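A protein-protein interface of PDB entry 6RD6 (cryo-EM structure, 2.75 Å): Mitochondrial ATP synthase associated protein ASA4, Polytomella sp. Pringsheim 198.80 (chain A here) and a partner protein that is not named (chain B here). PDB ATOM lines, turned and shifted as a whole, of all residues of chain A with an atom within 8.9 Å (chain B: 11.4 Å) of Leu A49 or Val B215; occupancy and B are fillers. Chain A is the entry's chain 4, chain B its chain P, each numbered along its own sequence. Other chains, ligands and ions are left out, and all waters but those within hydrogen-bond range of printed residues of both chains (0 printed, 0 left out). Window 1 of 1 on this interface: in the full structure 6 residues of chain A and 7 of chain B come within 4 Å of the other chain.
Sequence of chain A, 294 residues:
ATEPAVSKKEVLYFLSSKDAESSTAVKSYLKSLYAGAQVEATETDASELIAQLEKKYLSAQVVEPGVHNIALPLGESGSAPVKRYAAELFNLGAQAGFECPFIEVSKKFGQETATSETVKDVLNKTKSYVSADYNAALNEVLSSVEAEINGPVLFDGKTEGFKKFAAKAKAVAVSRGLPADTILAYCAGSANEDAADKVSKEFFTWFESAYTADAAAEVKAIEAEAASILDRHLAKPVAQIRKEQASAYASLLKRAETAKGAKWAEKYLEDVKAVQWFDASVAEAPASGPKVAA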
ATOM      1  N   ALA A  46     -15.361   1.896 -15.077  1.00  0.00           N
ATOM      2  CA  ALA A  46     -14.136   2.396 -15.752  1.00  0.00           C
ATOM      3  C   ALA A  46     -14.468   3.261 -16.977  1.00  0.00           C
ATOM      4  O   ALA A  46     -15.299   2.873 -17.822  1.00  0.00           O
ATOM      5  CB  ALA A  46     -13.138   1.299 -16.054  1.00  0.00           C
ATOM      6  N   SER A  47     -13.756   4.380 -17.119  1.00  0.00           N
ATOM      7  CA  SER A  47     -13.956   5.292 -18.276  1.00  0.00           C
ATOM      8  C   SER A  47     -13.364   4.661 -19.541  1.00  0.00           C
ATOM      9  O   SER A  47     -12.490   3.774 -19.422  1.00  0.00           O
ATOM     10  CB  SER A  47     -13.393   6.664 -18.011  1.00  0.00           C
ATOM     11  OG  SER A  47     -12.181   6.868 -18.722  1.00  0.00           O
ATOM     12  N   GLU A  48     -13.729   5.187 -20.713  1.00  0.00           N
ATOM     13  CA  GLU A  48     -13.262   4.593 -21.993  1.00  0.00           C
ATOM     14  C   GLU A  48     -11.729   4.573 -22.020  1.00  0.00           C
ATOM     15  O   GLU A  48     -11.196   3.512 -22.352  1.00  0.00           O
ATOM     16  CB  GLU A  48     -13.825   5.372 -23.182  1.00  0.00           C
ATOM     17  CG  GLU A  48     -13.714   6.877 -23.024  1.00  0.00           C
ATOM     18  CD  GLU A  48     -13.597   7.649 -24.327  1.00  0.00           C
ATOM     19  OE1 GLU A  48     -14.630   7.827 -25.003  1.00  0.00           O
ATOM     20  OE2 GLU A  48     -12.472   8.074 -24.661  1.00  0.00           O
ATOM     21  N   LEU A  49     -11.068   5.654 -21.589  1.00  0.00           N
ATOM     22  CA  LEU A  49      -9.583   5.721 -21.540  1.00  0.00           C
ATOM     23  C   LEU A  49      -9.036   4.667 -20.566  1.00  0.00           C
ATOM     24  O   LEU A  49      -7.972   4.101 -20.853  1.00  0.00           O
ATOM     25  CB  LEU A  49      -9.174   7.126 -21.089  1.00  0.00           C
ATOM     26  CG  LEU A  49      -9.191   8.201 -22.172  1.00  0.00           C
ATOM     27  CD1 LEU A  49      -8.912   9.568 -21.569  1.00  0.00           C
ATOM     28  CD2 LEU A  49      -8.179   7.885 -23.262  1.00  0.00           C
ATOM     29  N   ILE A  50      -9.670   4.488 -19.407  1.00  0.00           N
ATOM     30  CA  ILE A  50      -9.188   3.459 -18.436  1.00  0.00           C
ATOM     31  C   ILE A  50      -9.407   2.053 -19.008  1.00  0.00           C
ATOM     32  O   ILE A  50      -8.525   1.201 -18.824  1.00  0.00           O
ATOM     33  CB  ILE A  50      -9.842   3.614 -17.051  1.00  0.00           C
ATOM     34  CG1 ILE A  50      -9.103   4.646 -16.200  1.00  0.00           C
ATOM     35  CG2 ILE A  50      -9.896   2.268 -16.352  1.00  0.00           C
ATOM     36  CD1 ILE A  50      -8.103   4.034 -15.252  1.00  0.00           C
ATOM     37  N   ALA A  51     -10.553   1.833 -19.658  1.00  0.00           N
ATOM     38  CA  ALA A  51     -10.912   0.511 -20.221  1.00  0.00           C
ATOM     39  C   ALA A  51      -9.959   0.134 -21.359  1.00  0.00           C
ATOM     40  O   ALA A  51      -9.510  -1.019 -21.385  1.00  0.00           O
ATOM     41  CB  ALA A  51     -12.344   0.523 -20.686  1.00  0.00           C
ATOM     42  N   GLN A  52      -9.687   1.070 -22.270  1.00  0.00           N
ATOM     43  CA  GLN A  52      -8.779   0.799 -23.417  1.00  0.00           C
ATOM     44  C   GLN A  52      -7.363   0.514 -22.905  1.00  0.00           C
ATOM     45  O   GLN A  52      -6.705  -0.369 -23.477  1.00  0.00           O
ATOM     46  CB  GLN A  52      -8.834   1.923 -24.453  1.00  0.00           C
ATOM     47  CG  GLN A  52      -8.415   3.285 -23.922  1.00  0.00           C
ATOM     48  CD  GLN A  52      -8.571   4.361 -24.967  1.00  0.00           C
ATOM     49  OE1 GLN A  52      -7.614   4.752 -25.632  1.00  0.00           O
ATOM     50  NE2 GLN A  52      -9.790   4.849 -25.126  1.00  0.00           N
ATOM     51  N   LEU A  53      -6.794   1.152 -21.748  1.00  0.00           N
ATOM     52  CA  LEU A  53      -5.467   0.866 -21.208  1.00  0.00           C
ATOM     53  C   LEU A  53      -5.402  -0.539 -20.619  1.00  0.00           C
ATOM     54  O   LEU A  53      -4.407  -1.260 -20.801  1.00  0.00           O
ATOM     55  CB  LEU A  53      -5.098   1.909 -20.157  1.00  0.00           C
ATOM     56  CG  LEU A  53      -3.704   1.818 -19.550  1.00  0.00           C
ATOM     57  CD1 LEU A  53      -2.678   2.364 -20.514  1.00  0.00           C
ATOM     58  CD2 LEU A  53      -3.666   2.574 -18.247  1.00  0.00           C
ATOM     59  N   GLU A  54      -6.471  -0.954 -19.933  1.00  0.00           N
ATOM     60  CA  GLU A  54      -6.565  -2.310 -19.409  1.00  0.00           C
ATOM     61  C   GLU A  54      -6.600  -3.336 -20.534  1.00  0.00           C
ATOM     62  O   GLU A  54      -5.958  -4.387 -20.440  1.00  0.00           O
ATOM     63  CB  GLU A  54      -7.810  -2.426 -18.534  1.00  0.00           C
ATOM     64  CG  GLU A  54      -7.735  -3.464 -17.443  1.00  0.00           C
ATOM     65  CD  GLU A  54      -8.778  -3.242 -16.368  1.00  0.00           C
ATOM     66  OE1 GLU A  54      -9.630  -2.346 -16.545  1.00  0.00           O
ATOM     67  OE2 GLU A  54      -8.751  -3.960 -15.346  1.00  0.00           O
ATOM     68  N   LYS A  55      -7.328  -3.032 -21.613  1.00  0.00           N
ATOM     69  CA  LYS A  55      -7.382  -3.914 -22.774  1.00  0.00           C
ATOM     70  C   LYS A  55      -6.025  -4.020 -23.453  1.00  0.00           C
ATOM     71  O   LYS A  55      -5.628  -5.106 -23.891  1.00  0.00           O
ATOM     72  CB  LYS A  55      -8.441  -3.401 -23.749  1.00  0.00           C
ATOM     73  CG  LYS A  55      -8.477  -4.085 -25.104  1.00  0.00           C
ATOM     74  CD  LYS A  55      -9.815  -3.862 -25.782  1.00  0.00           C
ATOM     75  CE  LYS A  55      -9.994  -4.774 -26.982  1.00  0.00           C
ATOM     76  NZ  LYS A  55      -9.093  -4.398 -28.103  1.00  0.00           N
ATOM     77  N   LYS A  56      -5.284  -2.909 -23.508  1.00  0.00           N
ATOM     78  CA  LYS A  56      -3.950  -2.909 -24.099  1.00  0.00           C
ATOM     79  C   LYS A  56      -2.989  -3.782 -23.302  1.00  0.00           C
ATOM     80  O   LYS A  56      -2.241  -4.585 -23.875  1.00  0.00           O
ATOM     81  CB  LYS A  56      -3.439  -1.473 -24.185  1.00  0.00           C
ATOM     82  CG  LYS A  56      -1.973  -1.326 -24.500  1.00  0.00           C
ATOM     83  CD  LYS A  56      -1.549   0.116 -24.352  1.00  0.00           C
ATOM     84  CE  LYS A  56      -0.056   0.269 -24.483  1.00  0.00           C
ATOM     85  NZ  LYS A  56       0.332   1.696 -24.609  1.00  0.00           N
ATOM     86  N   TYR A  57      -3.033  -3.682 -21.975  1.00  0.00           N
ATOM     87  CA  TYR A  57      -2.100  -4.470 -21.173  1.00  0.00           C
ATOM     88  C   TYR A  57      -2.509  -5.939 -21.099  1.00  0.00           C
ATOM     89  O   TYR A  57      -1.646  -6.823 -21.050  1.00  0.00           O
ATOM     90  CB  TYR A  57      -1.950  -3.851 -19.791  1.00  0.00           C
ATOM     91  CG  TYR A  57      -0.886  -2.793 -19.811  1.00  0.00           C
ATOM     92  CD1 TYR A  57      -1.160  -1.527 -20.302  1.00  0.00           C
ATOM     93  CD2 TYR A  57       0.406  -3.073 -19.403  1.00  0.00           C
ATOM     94  CE1 TYR A  57      -0.190  -0.563 -20.353  1.00  0.00           C
ATOM     95  CE2 TYR A  57       1.385  -2.114 -19.448  1.00  0.00           C
ATOM     96  CZ  TYR A  57       1.080  -0.861 -19.925  1.00  0.00           C
ATOM     97  OH  TYR A  57       2.050   0.104 -19.978  1.00  0.00           O
ATOM     98  N   GLN A 111      -8.688   7.068 -35.524  1.00  0.00           N
ATOM     99  CA  GLN A 111      -8.603   7.581 -34.164  1.00  0.00           C
ATOM    100  C   GLN A 111      -7.605   8.728 -34.061  1.00  0.00           C
ATOM    101  O   GLN A 111      -7.860   9.718 -33.368  1.00  0.00           O
ATOM    102  CB  GLN A 111      -8.230   6.439 -33.219  1.00  0.00           C
ATOM    103  CG  GLN A 111      -7.847   6.844 -31.815  1.00  0.00           C
ATOM    104  CD  GLN A 111      -7.438   5.654 -30.969  1.00  0.00           C
ATOM    105  OE1 GLN A 111      -7.494   4.511 -31.419  1.00  0.00           O
ATOM    106  NE2 GLN A 111      -7.025   5.919 -29.735  1.00  0.00           N
ATOM    107  N   LYS B 192     -14.052  21.934 -32.998  1.00  0.00           N
ATOM    108  CA  LYS B 192     -14.170  20.486 -33.081  1.00  0.00           C
ATOM    109  C   LYS B 192     -12.854  19.777 -32.796  1.00  0.00           C
ATOM    110  O   LYS B 192     -12.848  18.549 -32.682  1.00  0.00           O
ATOM    111  CB  LYS B 192     -14.705  20.067 -34.449  1.00  0.00           C
ATOM    112  CG  LYS B 192     -16.157  20.434 -34.673  1.00  0.00           C
ATOM    113  CD  LYS B 192     -16.639  19.954 -36.028  1.00  0.00           C
ATOM    114  CE  LYS B 192     -16.795  18.441 -36.044  1.00  0.00           C
ATOM    115  NZ  LYS B 192     -17.915  17.995 -35.167  1.00  0.00           N
ATOM    116  N   LYS B 193     -11.743  20.512 -32.684  1.00  0.00           N
ATOM    117  CA  LYS B 193     -10.509  19.901 -32.197  1.00  0.00           C
ATOM    118  C   LYS B 193     -10.633  19.522 -30.728  1.00  0.00           C
ATOM    119  O   LYS B 193      -9.999  18.564 -30.271  1.00  0.00           O
ATOM    120  CB  LYS B 193      -9.322  20.835 -32.421  1.00  0.00           C
ATOM    121  CG  LYS B 193      -8.922  20.958 -33.877  1.00  0.00           C
ATOM    122  CD  LYS B 193      -7.681  21.810 -34.047  1.00  0.00           C
ATOM    123  CE  LYS B 193      -7.306  21.931 -35.514  1.00  0.00           C
ATOM    124  NZ  LYS B 193      -6.860  20.623 -36.068  1.00  0.00           N
ATOM    125  N   LEU B 194     -11.424  20.275 -29.972  1.00  0.00           N
ATOM    126  CA  LEU B 194     -11.955  19.768 -28.717  1.00  0.00           C
ATOM    127  C   LEU B 194     -12.862  18.588 -29.027  1.00  0.00           C
ATOM    128  O   LEU B 194     -13.698  18.665 -29.930  1.00  0.00           O
ATOM    129  CB  LEU B 194     -12.744  20.853 -27.989  1.00  0.00           C
ATOM    130  CG  LEU B 194     -12.107  21.835 -27.008  1.00  0.00           C
ATOM    131  CD1 LEU B 194     -11.090  22.734 -27.673  1.00  0.00           C
ATOM    132  CD2 LEU B 194     -13.206  22.658 -26.379  1.00  0.00           C
ATOM    133  N   LEU B 195     -12.693  17.485 -28.304  1.00  0.00           N
ATOM    134  CA  LEU B 195     -13.521  16.320 -28.596  1.00  0.00           C
ATOM    135  C   LEU B 195     -14.835  16.386 -27.832  1.00  0.00           C
ATOM    136  O   LEU B 195     -15.896  16.061 -28.377  1.00  0.00           O
ATOM    137  CB  LEU B 195     -12.762  15.035 -28.275  1.00  0.00           C
ATOM    138  CG  LEU B 195     -11.929  14.402 -29.392  1.00  0.00           C
ATOM    139  CD1 LEU B 195     -10.659  15.188 -29.668  1.00  0.00           C
ATOM    140  CD2 LEU B 195     -11.599  12.963 -29.041  1.00  0.00           C
ATOM    141  N   GLY B 196     -14.781  16.810 -26.578  1.00  0.00           N
ATOM    142  CA  GLY B 196     -15.968  17.008 -25.772  1.00  0.00           C
ATOM    143  C   GLY B 196     -15.637  17.996 -24.681  1.00  0.00           C
ATOM    144  O   GLY B 196     -14.582  18.631 -24.691  1.00  0.00           O
ATOM    145  N   GLY B 197     -16.556  18.119 -23.731  1.00  0.00           N
ATOM    146  CA  GLY B 197     -16.347  19.038 -22.634  1.00  0.00           C
ATOM    147  C   GLY B 197     -16.477  20.485 -23.074  1.00  0.00           C
ATOM    148  O   GLY B 197     -17.247  20.827 -23.975  1.00  0.00           O
ATOM    149  N   PHE B 198     -15.689  21.343 -22.430  1.00  0.00           N
ATOM    150  CA  PHE B 198     -15.735  22.771 -22.698  1.00  0.00           C
ATOM    151  C   PHE B 198     -14.425  23.424 -22.282  1.00  0.00           C
ATOM    152  O   PHE B 198     -13.672  22.892 -21.464  1.00  0.00           O
ATOM    153  CB  PHE B 198     -16.907  23.450 -21.975  1.00  0.00           C
ATOM    154  CG  PHE B 198     -17.043  23.064 -20.528  1.00  0.00           C
ATOM    155  CD1 PHE B 198     -17.880  22.026 -20.148  1.00  0.00           C
ATOM    156  CD2 PHE B 198     -16.355  23.756 -19.543  1.00  0.00           C
ATOM    157  CE1 PHE B 198     -18.012  21.676 -18.820  1.00  0.00           C
ATOM    158  CE2 PHE B 198     -16.485  23.411 -18.216  1.00  0.00           C
ATOM    159  CZ  PHE B 198     -17.315  22.371 -17.854  1.00  0.00           C
ATOM    160  N   ASP B 208      -9.742  24.533 -18.691  1.00  0.00           N
ATOM    161  CA  ASP B 208      -9.772  23.595 -19.811  1.00  0.00           C
ATOM    162  C   ASP B 208     -10.335  22.270 -19.316  1.00  0.00           C
ATOM    163  O   ASP B 208      -9.585  21.361 -18.953  1.00  0.00           O
ATOM    164  CB  ASP B 208      -8.376  23.421 -20.397  1.00  0.00           C
ATOM    165  CG  ASP B 208      -8.398  23.021 -21.853  1.00  0.00           C
ATOM    166  OD1 ASP B 208      -9.164  22.103 -22.209  1.00  0.00           O
ATOM    167  OD2 ASP B 208      -7.646  23.621 -22.647  1.00  0.00           O
ATOM    168  N   MET B 209     -11.663  22.153 -19.310  1.00  0.00           N
ATOM    169  CA  MET B 209     -12.325  20.898 -18.982  1.00  0.00           C
ATOM    170  C   MET B 209     -12.729  20.129 -20.231  1.00  0.00           C
ATOM    171  O   MET B 209     -13.721  19.394 -20.212  1.00  0.00           O
ATOM    172  CB  MET B 209     -13.538  21.142 -18.086  1.00  0.00           C
ATOM    173  CG  MET B 209     -13.170  21.634 -16.702  1.00  0.00           C
ATOM    174  SD  MET B 209     -14.575  21.871 -15.602  1.00  0.00           S
ATOM    175  CE  MET B 209     -15.035  20.173 -15.276  1.00  0.00           C
ATOM    176  N   SER B 210     -11.983  20.292 -21.318  1.00  0.00           N
ATOM    177  CA  SER B 210     -12.238  19.531 -22.528  1.00  0.00           C
ATOM    178  C   SER B 210     -11.735  18.104 -22.369  1.00  0.00           C
ATOM    179  O   SER B 210     -10.924  17.802 -21.491  1.00  0.00           O
ATOM    180  CB  SER B 210     -11.561  20.189 -23.724  1.00  0.00           C
ATOM    181  OG  SER B 210     -10.171  20.329 -23.500  1.00  0.00           O
ATOM    182  N   THR B 211     -12.227  17.216 -23.232  1.00  0.00           N
ATOM    183  CA  THR B 211     -11.799  15.826 -23.157  1.00  0.00           C
ATOM    184  C   THR B 211     -10.484  15.609 -23.891  1.00  0.00           C
ATOM    185  O   THR B 211      -9.797  14.613 -23.653  1.00  0.00           O
ATOM    186  CB  THR B 211     -12.880  14.898 -23.705  1.00  0.00           C
ATOM    187  OG1 THR B 211     -13.225  15.296 -25.033  1.00  0.00           O
ATOM    188  CG2 THR B 211     -14.116  14.946 -22.823  1.00  0.00           C
ATOM    189  N   ALA B 212     -10.112  16.527 -24.786  1.00  0.00           N
ATOM    190  CA  ALA B 212      -8.823  16.407 -25.463  1.00  0.00           C
ATOM    191  C   ALA B 212      -7.673  16.691 -24.506  1.00  0.00           C
ATOM    192  O   ALA B 212      -6.669  15.966 -24.490  1.00  0.00           O
ATOM    193  CB  ALA B 212      -8.771  17.349 -26.664  1.00  0.00           C
ATOM    194  N   LYS B 213      -7.817  17.731 -23.682  1.00  0.00           N
ATOM    195  CA  LYS B 213      -6.859  17.986 -22.612  1.00  0.00           C
ATOM    196  C   LYS B 213      -6.859  16.847 -21.600  1.00  0.00           C
ATOM    197  O   LYS B 213      -5.808  16.493 -21.055  1.00  0.00           O
ATOM    198  CB  LYS B 213      -7.183  19.320 -21.936  1.00  0.00           C
ATOM    199  CG  LYS B 213      -6.276  19.703 -20.776  1.00  0.00           C
ATOM    200  CD  LYS B 213      -4.828  19.785 -21.212  1.00  0.00           C
ATOM    201  CE  LYS B 213      -4.574  21.026 -22.047  1.00  0.00           C
ATOM    202  NZ  LYS B 213      -4.397  22.240 -21.205  1.00  0.00           N
ATOM    203  N   LYS B 214      -8.023  16.230 -21.380  1.00  0.00           N
ATOM    204  CA  LYS B 214      -8.115  15.113 -20.447  1.00  0.00           C
ATOM    205  C   LYS B 214      -7.367  13.888 -20.958  1.00  0.00           C
ATOM    206  O   LYS B 214      -6.633  13.249 -20.199  1.00  0.00           O
ATOM    207  CB  LYS B 214      -9.576  14.771 -20.181  1.00  0.00           C
ATOM    208  CG  LYS B 214      -9.760  13.699 -19.132  1.00  0.00           C
ATOM    209  CD  LYS B 214     -11.199  13.259 -19.059  1.00  0.00           C
ATOM    210  CE  LYS B 214     -11.362  12.130 -18.069  1.00  0.00           C
ATOM    211  NZ  LYS B 214     -10.978  12.541 -16.697  1.00  0.00           N
ATOM    212  N   VAL B 215      -7.516  13.553 -22.245  1.00  0.00           N
ATOM    213  CA  VAL B 215      -6.824  12.376 -22.763  1.00  0.00           C
ATOM    214  C   VAL B 215      -5.339  12.660 -22.937  1.00  0.00           C
ATOM    215  O   VAL B 215      -4.510  11.751 -22.828  1.00  0.00           O
ATOM    216  CB  VAL B 215      -7.471  11.864 -24.068  1.00  0.00           C
ATOM    217  CG1 VAL B 215      -8.913  11.462 -23.832  1.00  0.00           C
ATOM    218  CG2 VAL B 215      -7.371  12.864 -25.193  1.00  0.00           C
ATOM    219  N   GLU B 216      -4.964  13.928 -23.138  1.00  0.00           N
ATOM    220  CA  GLU B 216      -3.542  14.248 -23.224  1.00  0.00           C
ATOM    221  C   GLU B 216      -2.877  14.183 -21.851  1.00  0.00           C
ATOM    222  O   GLU B 216      -1.754  13.674 -21.720  1.00  0.00           O
ATOM    223  CB  GLU B 216      -3.361  15.624 -23.856  1.00  0.00           C
ATOM    224  CG  GLU B 216      -1.921  16.004 -24.114  1.00  0.00           C
ATOM    225  CD  GLU B 216      -1.796  17.330 -24.830  1.00  0.00           C
ATOM    226  OE1 GLU B 216      -2.842  17.955 -25.104  1.00  0.00           O
ATOM    227  OE2 GLU B 216      -0.656  17.743 -25.123  1.00  0.00           O
ATOM    228  N   GLU B 217      -3.574  14.655 -20.812  1.00  0.00           N
ATOM    229  CA  GLU B 217      -3.084  14.511 -19.445  1.00  0.00           C
ATOM    230  C   GLU B 217      -3.045  13.047 -19.026  1.00  0.00           C
ATOM    231  O   GLU B 217      -2.128  12.624 -18.312  1.00  0.00           O
ATOM    232  CB  GLU B 217      -3.968  15.312 -18.492  1.00  0.00           C
ATOM    233  CG  GLU B 217      -3.712  16.808 -18.498  1.00  0.00           C
ATOM    234  CD  GLU B 217      -2.357  17.176 -17.940  1.00  0.00           C
ATOM    235  OE1 GLU B 217      -2.167  17.045 -16.713  1.00  0.00           O
ATOM    236  OE2 GLU B 217      -1.481  17.596 -18.725  1.00  0.00           O
ATOM    237  N   PHE B 218      -4.034  12.264 -19.474  1.00  0.00           N
ATOM    238  CA  PHE B 218      -4.064  10.822 -19.250  1.00  0.00           C
ATOM    239  C   PHE B 218      -2.852  10.139 -19.862  1.00  0.00           C
ATOM    240  O   PHE B 218      -2.203   9.315 -19.207  1.00  0.00           O
ATOM    241  CB  PHE B 218      -5.356  10.254 -19.840  1.00  0.00           C
ATOM    242  CG  PHE B 218      -5.552   8.779 -19.621  1.00  0.00           C
ATOM    243  CD1 PHE B 218      -5.144   7.851 -20.573  1.00  0.00           C
ATOM    244  CD2 PHE B 218      -6.190   8.323 -18.487  1.00  0.00           C
ATOM    245  CE1 PHE B 218      -5.334   6.504 -20.371  1.00  0.00           C
ATOM    246  CE2 PHE B 218      -6.394   6.979 -18.294  1.00  0.00           C
ATOM    247  CZ  PHE B 218      -5.958   6.069 -19.230  1.00  0.00           C
ATOM    248  N   ASN B 219      -2.544  10.467 -21.119  1.00  0.00           N
ATOM    249  CA  ASN B 219      -1.421   9.837 -21.800  1.00  0.00           C
ATOM    250  C   ASN B 219      -0.099  10.239 -21.166  1.00  0.00           C
ATOM    251  O   ASN B 219       0.798   9.403 -21.019  1.00  0.00           O
ATOM    252  CB  ASN B 219      -1.442  10.195 -23.283  1.00  0.00           C
ATOM    253  CG  ASN B 219      -2.595   9.551 -24.016  1.00  0.00           C
ATOM    254  OD1 ASN B 219      -3.077   8.490 -23.626  1.00  0.00           O
ATOM    255  ND2 ASN B 219      -3.044  10.190 -25.087  1.00  0.00           N
ATOM    256  N   ASN B 220       0.021  11.501 -20.739  1.00  0.00           N
ATOM    257  CA  ASN B 220       1.247  11.939 -20.076  1.00  0.00           C
ATOM    258  C   ASN B 220       1.426  11.264 -18.720  1.00  0.00           C
ATOM    259  O   ASN B 220       2.541  10.862 -18.365  1.00  0.00           O
ATOM    260  CB  ASN B 220       1.246  13.459 -19.927  1.00  0.00           C
ATOM    261  CG  ASN B 220       1.390  14.169 -21.253  1.00  0.00           C
ATOM    262  OD1 ASN B 220       1.011  15.330 -21.393  1.00  0.00           O
ATOM    263  ND2 ASN B 220       1.935  13.470 -22.239  1.00  0.00           N
ATOM    264  N   PHE B 221       0.335  11.094 -17.969  1.00  0.00           N
ATOM    265  CA  PHE B 221       0.416  10.441 -16.666  1.00  0.00           C
ATOM    266  C   PHE B 221       0.752   8.958 -16.806  1.00  0.00           C
ATOM    267  O   PHE B 221       1.557   8.415 -16.035  1.00  0.00           O
ATOM    268  CB  PHE B 221      -0.903  10.627 -15.922  1.00  0.00           C
ATOM    269  CG  PHE B 221      -0.944   9.956 -14.590  1.00  0.00           C
ATOM    270  CD1 PHE B 221      -0.222  10.462 -13.526  1.00  0.00           C
ATOM    271  CD2 PHE B 221      -1.709   8.820 -14.399  1.00  0.00           C
ATOM    272  CE1 PHE B 221      -0.258   9.846 -12.296  1.00  0.00           C
ATOM    273  CE2 PHE B 221      -1.749   8.200 -13.173  1.00  0.00           C
ATOM    274  CZ  PHE B 221      -1.024   8.714 -12.120  1.00  0.00           C
ATOM    275  N   VAL B 222       0.154   8.294 -17.799  1.00  0.00           N
ATOM    276  CA  VAL B 222       0.425   6.880 -18.040  1.00  0.00           C
ATOM    277  C   VAL B 222       1.866   6.681 -18.490  1.00  0.00           C
ATOM    278  O   VAL B 222       2.554   5.759 -18.025  1.00  0.00           O
ATOM    279  CB  VAL B 222      -0.590   6.322 -19.059  1.00  0.00           C
ATOM    280  CG1 VAL B 222      -0.103   5.033 -19.702  1.00  0.00           C
ATOM    281  CG2 VAL B 222      -1.921   6.090 -18.385  1.00  0.00           C
ATOM    282  N   ASN B 223       2.367   7.576 -19.350  1.00  0.00           N
ATOM    283  CA  ASN B 223       3.749   7.481 -19.807  1.00  0.00           C
ATOM    284  C   ASN B 223       4.737   7.729 -18.673  1.00  0.00           C
ATOM    285  O   ASN B 223       5.753   7.029 -18.567  1.00  0.00           O
ATOM    286  CB  ASN B 223       3.991   8.460 -20.951  1.00  0.00           C
ATOM    287  CG  ASN B 223       3.303   8.037 -22.227  1.00  0.00           C
ATOM    288  OD1 ASN B 223       2.936   8.871 -23.052  1.00  0.00           O
ATOM    289  ND2 ASN B 223       3.109   6.737 -22.389  1.00  0.00           N
ATOM    290  N   LYS B 224       4.440   8.691 -17.793  1.00  0.00           N
ATOM    291  CA  LYS B 224       5.337   8.948 -16.670  1.00  0.00           C
ATOM    292  C   LYS B 224       5.322   7.804 -15.660  1.00  0.00           C
ATOM    293  O   LYS B 224       6.358   7.503 -15.056  1.00  0.00           O
ATOM    294  CB  LYS B 224       4.989  10.277 -16.000  1.00  0.00           C
ATOM    295  CG  LYS B 224       5.373  11.492 -16.833  1.00  0.00           C
ATOM    296  CD  LYS B 224       5.248  12.790 -16.049  1.00  0.00           C
ATOM    297  CE  LYS B 224       3.799  13.203 -15.864  1.00  0.00           C
ATOM    298  NZ  LYS B 224       3.687  14.537 -15.215  1.00  0.00           N
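No residue of chain B comes within 4 Å of Glu A48. Leu A49 touches just these residues of chain B: Val B215 and Phe B218. No residue of chain B comes within 4 Å of Ile A50. No residue of chain B comes within 4 Å of Ala A51. No residue of chain B comes within 4 Å of Gln A52. Of chain B, only Val B222 (3.8 Å) comes within 4 Å of Leu A53. Of chain A, only Leu A49 (3.0 Å) comes within 4 Å of Val B215. Printed residues of chain A within 4 Å of Phe B218: Leu A49. Printed residues of chain A within 4 Å of Val B222: Leu A53. The nearest residue of chain B that does not touch Leu A49 is Lys B214 (4.5 Å). The nearest residue of chain A that does not touch Val B215 is Glu A48 (5.0 Å). The nearest printed residue of chain A that does not touch Val B222 is Tyr A57 (5.4 Å).
Of the 24 printed residues of chain B, 3 touch a printed residue of chain A. Hydrophobic or aromatic side chains of chain B that line the printed part of chain A: Val B215, Phe B218 and Val B222. Of the 13 printed residues of chain A, 2 touch a printed residue of chain B. Among the printed residues, no Asp or Glu carboxylate lies within 4 Å of a Lys or Arg side-chain nitrogen of the other chain.
OG of Ser A47 lies close to N of Leu A49, 3.3 Å away. ND2 of Asn B219 sits at hydrogen-bond distance from O of Val B215 (3.1 Å).
CD1 of Leu A49 touches CG1 of Val B215 (3.0 Å). O of Leu A49 touches CZ of Phe B218 (3.3 Å). Leu A53 touches Val B222.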
